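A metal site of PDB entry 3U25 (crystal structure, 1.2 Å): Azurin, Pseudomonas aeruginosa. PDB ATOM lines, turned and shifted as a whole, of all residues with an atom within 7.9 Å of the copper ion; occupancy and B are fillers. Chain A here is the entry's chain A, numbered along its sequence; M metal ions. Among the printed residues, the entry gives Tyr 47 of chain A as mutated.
The copper ion is bound by ND1 of His 116 (2.0 Å), ND1 of His 45 (2.1 Å) and SG of Cys 111 (2.2 Å). The copper ion has three donor atoms within binding distance.
Gly 44 touches the copper ion. Phe 113 touches the copper ion (CB to CU, 3.9 Å). SD of Met 120 touches the copper ion, 3.2 Å away. Of the 24 residues printed, 6 come within 4 Å of the copper ion. The nearest printed residue that does not touch the copper ion is Asn 46 (4.6 Å).
A ring nitrogen (ND1) of His 116 sits close to the backbone carbonyl oxygen of Gly 44 (3.5 Å). The side-chain sulfur (SD) of Met 12 sits close to a ring nitrogen (NE2) of His 116. O of Asn 9 lies within hydrogen-bond range of NE2 of His 45, at 2.8 Å. The backbone NH (N) of Phe 113 lies close to the side-chain sulfur (SG) of Cys 111, at 3.4 Å. ND1 of His 116 sits close to SD of Met 120 (3.7 Å). SD of Met 120 lies close to ND1 of His 45 (3.3 Å). The backbone carbonyl oxygen of Met 120 sits at hydrogen-bond distance from the backbone NH of Cys 111, at 3.1 Å. O of His 45 is in hydrogen-bond range of N of Ile 86 (2.8 Å).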
ATOM      1  N   GLY A   8     -11.768  21.307 -14.321  1.00  0.00           N
ATOM      2  CA  GLY A   8     -12.202  22.264 -13.301  1.00  0.00           C
ATOM      3  C   GLY A   8     -11.090  22.437 -12.293  1.00  0.00           C
ATOM      4  O   GLY A   8     -10.359  21.505 -12.016  1.00  0.00           O
ATOM      5  N   ASN A   9     -10.928  23.668 -11.753  1.00  0.00           N
ATOM      6  CA  ASN A   9      -9.727  23.942 -10.912  1.00  0.00           C
ATOM      7  C   ASN A   9     -10.060  24.436  -9.533  1.00  0.00           C
ATOM      8  O   ASN A   9     -11.235  24.558  -9.116  1.00  0.00           O
ATOM      9  CB  ASN A   9      -8.743  24.847 -11.652  1.00  0.00           C
ATOM     10  CG  ASN A   9      -9.243  26.270 -11.827  1.00  0.00           C
ATOM     11  OD1 ASN A   9     -10.179  26.694 -11.150  1.00  0.00           O
ATOM     12  ND2 ASN A   9      -8.515  27.044 -12.690  1.00  0.00           N
ATOM     13  N   MET A  12     -12.361  27.678  -8.999  1.00  0.00           N
ATOM     14  CA  MET A  12     -13.754  27.679  -9.490  1.00  0.00           C
ATOM     15  C   MET A  12     -13.836  28.105 -10.920  1.00  0.00           C
ATOM     16  O   MET A  12     -14.714  28.901 -11.269  1.00  0.00           O
ATOM     17  CB  MET A  12     -14.711  28.555  -8.649  1.00  0.00           C
ATOM     18  CG  MET A  12     -14.894  28.052  -7.233  1.00  0.00           C
ATOM     19  SD  MET A  12     -15.974  29.067  -6.192  1.00  0.00           S
ATOM     20  CE  MET A  12     -16.923  29.243  -7.234  1.00  0.00           C
ATOM     21  N   GLN A  13     -13.010  27.533 -11.762  1.00  0.00           N
ATOM     22  CA  GLN A  13     -13.051  27.749 -13.200  1.00  0.00           C
ATOM     23  C   GLN A  13     -13.026  26.458 -13.977  1.00  0.00           C
ATOM     24  O   GLN A  13     -12.199  25.591 -13.640  1.00  0.00           O
ATOM     25  CB  GLN A  13     -11.865  28.572 -13.683  1.00  0.00           C
ATOM     26  CG  GLN A  13     -11.665  29.889 -12.971  1.00  0.00           C
ATOM     27  CD  GLN A  13     -10.307  30.470 -13.347  1.00  0.00           C
ATOM     28  OE1 GLN A  13      -9.233  29.889 -13.116  1.00  0.00           O
ATOM     29  NE2 GLN A  13     -10.371  31.589 -14.099  1.00  0.00           N
ATOM     30  N   PHE A  14     -13.819  26.401 -15.038  1.00  0.00           N
ATOM     31  CA  PHE A  14     -13.546  25.452 -16.125  1.00  0.00           C
ATOM     32  C   PHE A  14     -12.506  26.017 -17.066  1.00  0.00           C
ATOM     33  O   PHE A  14     -12.385  27.275 -17.153  1.00  0.00           O
ATOM     34  CB  PHE A  14     -14.797  25.127 -16.994  1.00  0.00           C
ATOM     35  CG  PHE A  14     -15.880  24.299 -16.316  1.00  0.00           C
ATOM     36  CD1 PHE A  14     -15.573  23.040 -15.755  1.00  0.00           C
ATOM     37  CD2 PHE A  14     -17.205  24.744 -16.318  1.00  0.00           C
ATOM     38  CE1 PHE A  14     -16.578  22.230 -15.257  1.00  0.00           C
ATOM     39  CE2 PHE A  14     -18.193  23.912 -15.789  1.00  0.00           C
ATOM     40  CZ  PHE A  14     -17.876  22.658 -15.267  1.00  0.00           C
ATOM     41  N   LEU A  32     -13.994  14.878 -17.964  1.00  0.00           N
ATOM     42  CA  LEU A  32     -13.745  15.893 -16.943  1.00  0.00           C
ATOM     43  C   LEU A  32     -12.661  15.465 -16.027  1.00  0.00           C
ATOM     44  O   LEU A  32     -12.597  14.294 -15.612  1.00  0.00           O
ATOM     45  CB  LEU A  32     -15.027  16.160 -16.114  1.00  0.00           C
ATOM     46  CG  LEU A  32     -14.920  17.282 -15.093  1.00  0.00           C
ATOM     47  CD1 LEU A  32     -14.807  18.666 -15.746  1.00  0.00           C
ATOM     48  CD2 LEU A  32     -16.150  17.266 -14.205  1.00  0.00           C
ATOM     49  N   HIS A  34     -10.004  17.012 -12.556  1.00  0.00           N
ATOM     50  CA  HIS A  34      -9.797  18.011 -11.476  1.00  0.00           C
ATOM     51  C   HIS A  34      -8.347  17.959 -11.108  1.00  0.00           C
ATOM     52  O   HIS A  34      -7.941  17.139 -10.230  1.00  0.00           O
ATOM     53  CB  HIS A  34     -10.682  17.697 -10.304  1.00  0.00           C
ATOM     54  CG  HIS A  34     -10.738  18.779  -9.278  1.00  0.00           C
ATOM     55  ND1 HIS A  34      -9.650  19.603  -8.936  1.00  0.00           N
ATOM     56  CD2 HIS A  34     -11.802  19.202  -8.581  1.00  0.00           C
ATOM     57  CE1 HIS A  34     -10.083  20.379  -7.929  1.00  0.00           C
ATOM     58  NE2 HIS A  34     -11.383  20.217  -7.746  1.00  0.00           N
ATOM     59  N   VAL A  42     -15.051  20.645  -0.605  1.00  0.00           N
ATOM     60  CA  VAL A  42     -14.979  22.116  -0.641  1.00  0.00           C
ATOM     61  C   VAL A  42     -14.814  22.667  -2.022  1.00  0.00           C
ATOM     62  O   VAL A  42     -14.995  23.878  -2.205  1.00  0.00           O
ATOM     63  CB  VAL A  42     -13.877  22.695   0.315  1.00  0.00           C
ATOM     64  CG1 VAL A  42     -14.103  22.254   1.750  1.00  0.00           C
ATOM     65  CG2 VAL A  42     -12.518  22.269  -0.138  1.00  0.00           C
ATOM     66  N   MET A  43     -14.504  21.858  -3.042  1.00  0.00           N
ATOM     67  CA  MET A  43     -14.205  22.330  -4.382  1.00  0.00           C
ATOM     68  C   MET A  43     -14.513  21.186  -5.339  1.00  0.00           C
ATOM     69  O   MET A  43     -13.827  20.978  -6.342  1.00  0.00           O
ATOM     70  CB  MET A  43     -12.741  22.723  -4.485  1.00  0.00           C
ATOM     71  CG  MET A  43     -12.367  23.525  -5.739  1.00  0.00           C
ATOM     72  SD  MET A  43     -13.374  25.026  -6.048  1.00  0.00           S
ATOM     73  CE  MET A  43     -12.934  26.022  -4.635  1.00  0.00           C
ATOM     74  N   GLY A  44     -15.690  20.577  -5.145  1.00  0.00           N
ATOM     75  CA  GLY A  44     -16.131  19.547  -6.074  1.00  0.00           C
ATOM     76  C   GLY A  44     -16.642  20.210  -7.334  1.00  0.00           C
ATOM     77  O   GLY A  44     -17.296  21.252  -7.303  1.00  0.00           O
ATOM     78  N   HIS A  45     -16.433  19.519  -8.471  1.00  0.00           N
ATOM     79  CA  HIS A  45     -16.980  19.958  -9.773  1.00  0.00           C
ATOM     80  C   HIS A  45     -17.682  18.840 -10.537  1.00  0.00           C
ATOM     81  O   HIS A  45     -17.160  17.666 -10.475  1.00  0.00           O
ATOM     82  CB  HIS A  45     -15.892  20.571 -10.678  1.00  0.00           C
ATOM     83  CG  HIS A  45     -15.104  21.669 -10.116  1.00  0.00           C
ATOM     84  ND1 HIS A  45     -15.664  22.772  -9.529  1.00  0.00           N
ATOM     85  CD2 HIS A  45     -13.770  21.808 -10.024  1.00  0.00           C
ATOM     86  CE1 HIS A  45     -14.675  23.621  -9.191  1.00  0.00           C
ATOM     87  NE2 HIS A  45     -13.538  23.037  -9.390  1.00  0.00           N
ATOM     88  N   ASN A  46     -18.765  19.196 -11.175  1.00  0.00           N
ATOM     89  CA  ASN A  46     -19.354  18.299 -12.175  1.00  0.00           C
ATOM     90  C   ASN A  46     -19.547  19.046 -13.445  1.00  0.00           C
ATOM     91  O   ASN A  46     -19.375  20.271 -13.526  1.00  0.00           O
ATOM     92  CB  ASN A  46     -20.641  17.611 -11.610  1.00  0.00           C
ATOM     93  CG  ASN A  46     -21.664  18.587 -11.107  1.00  0.00           C
ATOM     94  OD1 ASN A  46     -21.576  19.814 -11.320  1.00  0.00           O
ATOM     95  ND2 ASN A  46     -22.627  18.112 -10.352  1.00  0.00           N
ATOM     96  N   TYR A  47     -19.743  18.262 -14.495  1.00  0.00           N
ATOM     97  CA  TYR A  47     -20.202  18.774 -15.793  1.00  0.00           C
ATOM     98  C   TYR A  47     -21.613  18.326 -15.964  1.00  0.00           C
ATOM     99  O   TYR A  47     -21.906  17.089 -16.033  1.00  0.00           O
ATOM    100  CB  TYR A  47     -19.278  18.298 -16.913  1.00  0.00           C
ATOM    101  CG  TYR A  47     -19.702  18.593 -18.315  1.00  0.00           C
ATOM    102  CD1 TYR A  47     -19.097  19.644 -19.061  1.00  0.00           C
ATOM    103  CD2 TYR A  47     -20.729  17.832 -18.939  1.00  0.00           C
ATOM    104  CE1 TYR A  47     -19.468  19.832 -20.405  1.00  0.00           C
ATOM    105  CE2 TYR A  47     -21.113  18.110 -20.242  1.00  0.00           C
ATOM    106  CZ  TYR A  47     -20.519  19.082 -20.943  1.00  0.00           C
ATOM    107  OH  TYR A  47     -20.948  19.283 -22.247  1.00  0.00           O
ATOM    108  N   LEU A  85     -19.623  14.234  -9.578  1.00  0.00           N
ATOM    109  CA  LEU A  85     -18.920  15.332  -8.867  1.00  0.00           C
ATOM    110  C   LEU A  85     -17.568  14.785  -8.498  1.00  0.00           C
ATOM    111  O   LEU A  85     -17.493  13.723  -7.844  1.00  0.00           O
ATOM    112  CB  LEU A  85     -19.708  15.719  -7.618  1.00  0.00           C
ATOM    113  CG  LEU A  85     -19.252  16.986  -6.910  1.00  0.00           C
ATOM    114  CD1 LEU A  85     -19.706  18.231  -7.713  1.00  0.00           C
ATOM    115  CD2 LEU A  85     -19.715  17.098  -5.454  1.00  0.00           C
ATOM    116  N   ILE A  86     -16.492  15.476  -8.833  1.00  0.00           N
ATOM    117  CA  ILE A  86     -15.134  15.019  -8.575  1.00  0.00           C
ATOM    118  C   ILE A  86     -14.355  16.093  -7.799  1.00  0.00           C
ATOM    119  O   ILE A  86     -14.573  17.321  -7.921  1.00  0.00           O
ATOM    120  CB  ILE A  86     -14.399  14.659  -9.889  1.00  0.00           C
ATOM    121  CG1 ILE A  86     -14.300  15.856 -10.834  1.00  0.00           C
ATOM    122  CG2 ILE A  86     -15.086  13.452 -10.535  1.00  0.00           C
ATOM    123  CD1 ILE A  86     -13.445  15.541 -12.088  1.00  0.00           C
ATOM    124  N   PHE A 110     -22.549  23.228 -17.011  1.00  0.00           N
ATOM    125  CA  PHE A 110     -22.295  23.948 -15.783  1.00  0.00           C
ATOM    126  C   PHE A 110     -21.960  22.980 -14.658  1.00  0.00           C
ATOM    127  O   PHE A 110     -22.264  21.768 -14.723  1.00  0.00           O
ATOM    128  CB  PHE A 110     -23.507  24.820 -15.456  1.00  0.00           C
ATOM    129  CG  PHE A 110     -24.811  24.066 -15.511  1.00  0.00           C
ATOM    130  CD1 PHE A 110     -25.489  23.976 -16.724  1.00  0.00           C
ATOM    131  CD2 PHE A 110     -25.370  23.458 -14.398  1.00  0.00           C
ATOM    132  CE1 PHE A 110     -26.659  23.224 -16.830  1.00  0.00           C
ATOM    133  CE2 PHE A 110     -26.544  22.733 -14.485  1.00  0.00           C
ATOM    134  CZ  PHE A 110     -27.178  22.648 -15.736  1.00  0.00           C
ATOM    135  N   CYS A 111     -21.440  23.555 -13.580  1.00  0.00           N
ATOM    136  CA  CYS A 111     -21.240  22.869 -12.318  1.00  0.00           C
ATOM    137  C   CYS A 111     -22.332  23.229 -11.339  1.00  0.00           C
ATOM    138  O   CYS A 111     -22.722  24.403 -11.285  1.00  0.00           O
ATOM    139  CB  CYS A 111     -19.911  23.269 -11.789  1.00  0.00           C
ATOM    140  SG  CYS A 111     -19.522  22.472 -10.160  1.00  0.00           S
ATOM    141  N   THR A 112     -22.880  22.231 -10.597  1.00  0.00           N
ATOM    142  CA  THR A 112     -23.929  22.551  -9.640  1.00  0.00           C
ATOM    143  C   THR A 112     -23.449  22.643  -8.160  1.00  0.00           C
ATOM    144  O   THR A 112     -24.280  22.772  -7.274  1.00  0.00           O
ATOM    145  CB  THR A 112     -25.087  21.501  -9.697  1.00  0.00           C
ATOM    146  OG1 THR A 112     -24.551  20.196  -9.385  1.00  0.00           O
ATOM    147  CG2 THR A 112     -25.770  21.490 -11.039  1.00  0.00           C
ATOM    148  N   PHE A 113     -22.128  22.535  -7.940  1.00  0.00           N
ATOM    149  CA  PHE A 113     -21.669  22.738  -6.550  1.00  0.00           C
ATOM    150  C   PHE A 113     -22.131  24.149  -6.104  1.00  0.00           C
ATOM    151  O   PHE A 113     -22.015  25.105  -6.840  1.00  0.00           O
ATOM    152  CB  PHE A 113     -20.190  22.582  -6.505  1.00  0.00           C
ATOM    153  CG  PHE A 113     -19.608  22.402  -5.137  1.00  0.00           C
ATOM    154  CD1 PHE A 113     -19.366  23.511  -4.319  1.00  0.00           C
ATOM    155  CD2 PHE A 113     -19.386  21.156  -4.681  1.00  0.00           C
ATOM    156  CE1 PHE A 113     -18.883  23.278  -2.962  1.00  0.00           C
ATOM    157  CE2 PHE A 113     -18.811  20.930  -3.378  1.00  0.00           C
ATOM    158  CZ  PHE A 113     -18.549  21.936  -2.558  1.00  0.00           C
ATOM    159  N   PRO A 114     -22.568  24.287  -4.831  1.00  0.00           N
ATOM    160  CA  PRO A 114     -22.939  25.589  -4.303  1.00  0.00           C
ATOM    161  C   PRO A 114     -21.950  26.716  -4.629  1.00  0.00           C
ATOM    162  O   PRO A 114     -20.762  26.594  -4.384  1.00  0.00           O
ATOM    163  CB  PRO A 114     -23.118  25.407  -2.808  1.00  0.00           C
ATOM    164  CG  PRO A 114     -23.628  23.936  -2.753  1.00  0.00           C
ATOM    165  CD  PRO A 114     -22.833  23.238  -3.835  1.00  0.00           C
ATOM    166  N   GLY A 115     -22.481  27.791  -5.253  1.00  0.00           N
ATOM    167  CA  GLY A 115     -21.623  28.953  -5.512  1.00  0.00           C
ATOM    168  C   GLY A 115     -20.838  28.904  -6.826  1.00  0.00           C
ATOM    169  O   GLY A 115     -20.097  29.864  -7.115  1.00  0.00           O
ATOM    170  N   HIS A 116     -20.832  27.749  -7.535  1.00  0.00           N
ATOM    171  CA  HIS A 116     -19.909  27.596  -8.714  1.00  0.00           C
ATOM    172  C   HIS A 116     -20.587  27.927  -9.992  1.00  0.00           C
ATOM    173  O   HIS A 116     -19.880  28.357 -10.903  1.00  0.00           O
ATOM    174  CB  HIS A 116     -19.424  26.154  -8.790  1.00  0.00           C
ATOM    175  CG  HIS A 116     -18.491  25.756  -7.714  1.00  0.00           C
ATOM    176  ND1 HIS A 116     -17.668  24.642  -7.858  1.00  0.00           N
ATOM    177  CD2 HIS A 116     -18.225  26.343  -6.510  1.00  0.00           C
ATOM    178  CE1 HIS A 116     -16.959  24.540  -6.729  1.00  0.00           C
ATOM    179  NE2 HIS A 116     -17.288  25.547  -5.901  1.00  0.00           N
ATOM    180  N   SER A 117     -21.902  27.818 -10.111  1.00  0.00           N
ATOM    181  CA  SER A 117     -22.526  27.835 -11.523  1.00  0.00           C
ATOM    182  C   SER A 117     -22.348  29.077 -12.264  1.00  0.00           C
ATOM    183  O   SER A 117     -22.129  29.017 -13.496  1.00  0.00           O
ATOM    184  CB  SER A 117     -23.970  27.438 -11.472  1.00  0.00           C
ATOM    185  OG  SER A 117     -24.770  28.400 -10.721  1.00  0.00           O
ATOM    186  N   MET A 120     -18.817  28.816 -13.426  1.00  0.00           N
ATOM    187  CA  MET A 120     -18.495  27.544 -14.143  1.00  0.00           C
ATOM    188  C   MET A 120     -19.682  27.151 -15.036  1.00  0.00           C
ATOM    189  O   MET A 120     -20.474  26.308 -14.619  1.00  0.00           O
ATOM    190  CB  MET A 120     -18.182  26.492 -13.093  1.00  0.00           C
ATOM    191  CG  MET A 120     -16.908  26.919 -12.279  1.00  0.00           C
ATOM    192  SD  MET A 120     -16.374  25.529 -11.197  1.00  0.00           S
ATOM    193  CE  MET A 120     -15.776  24.399 -12.425  1.00  0.00           C
HETATM  194 CU    CU M   1     -17.667  23.277  -9.351  1.00  0.00          CU
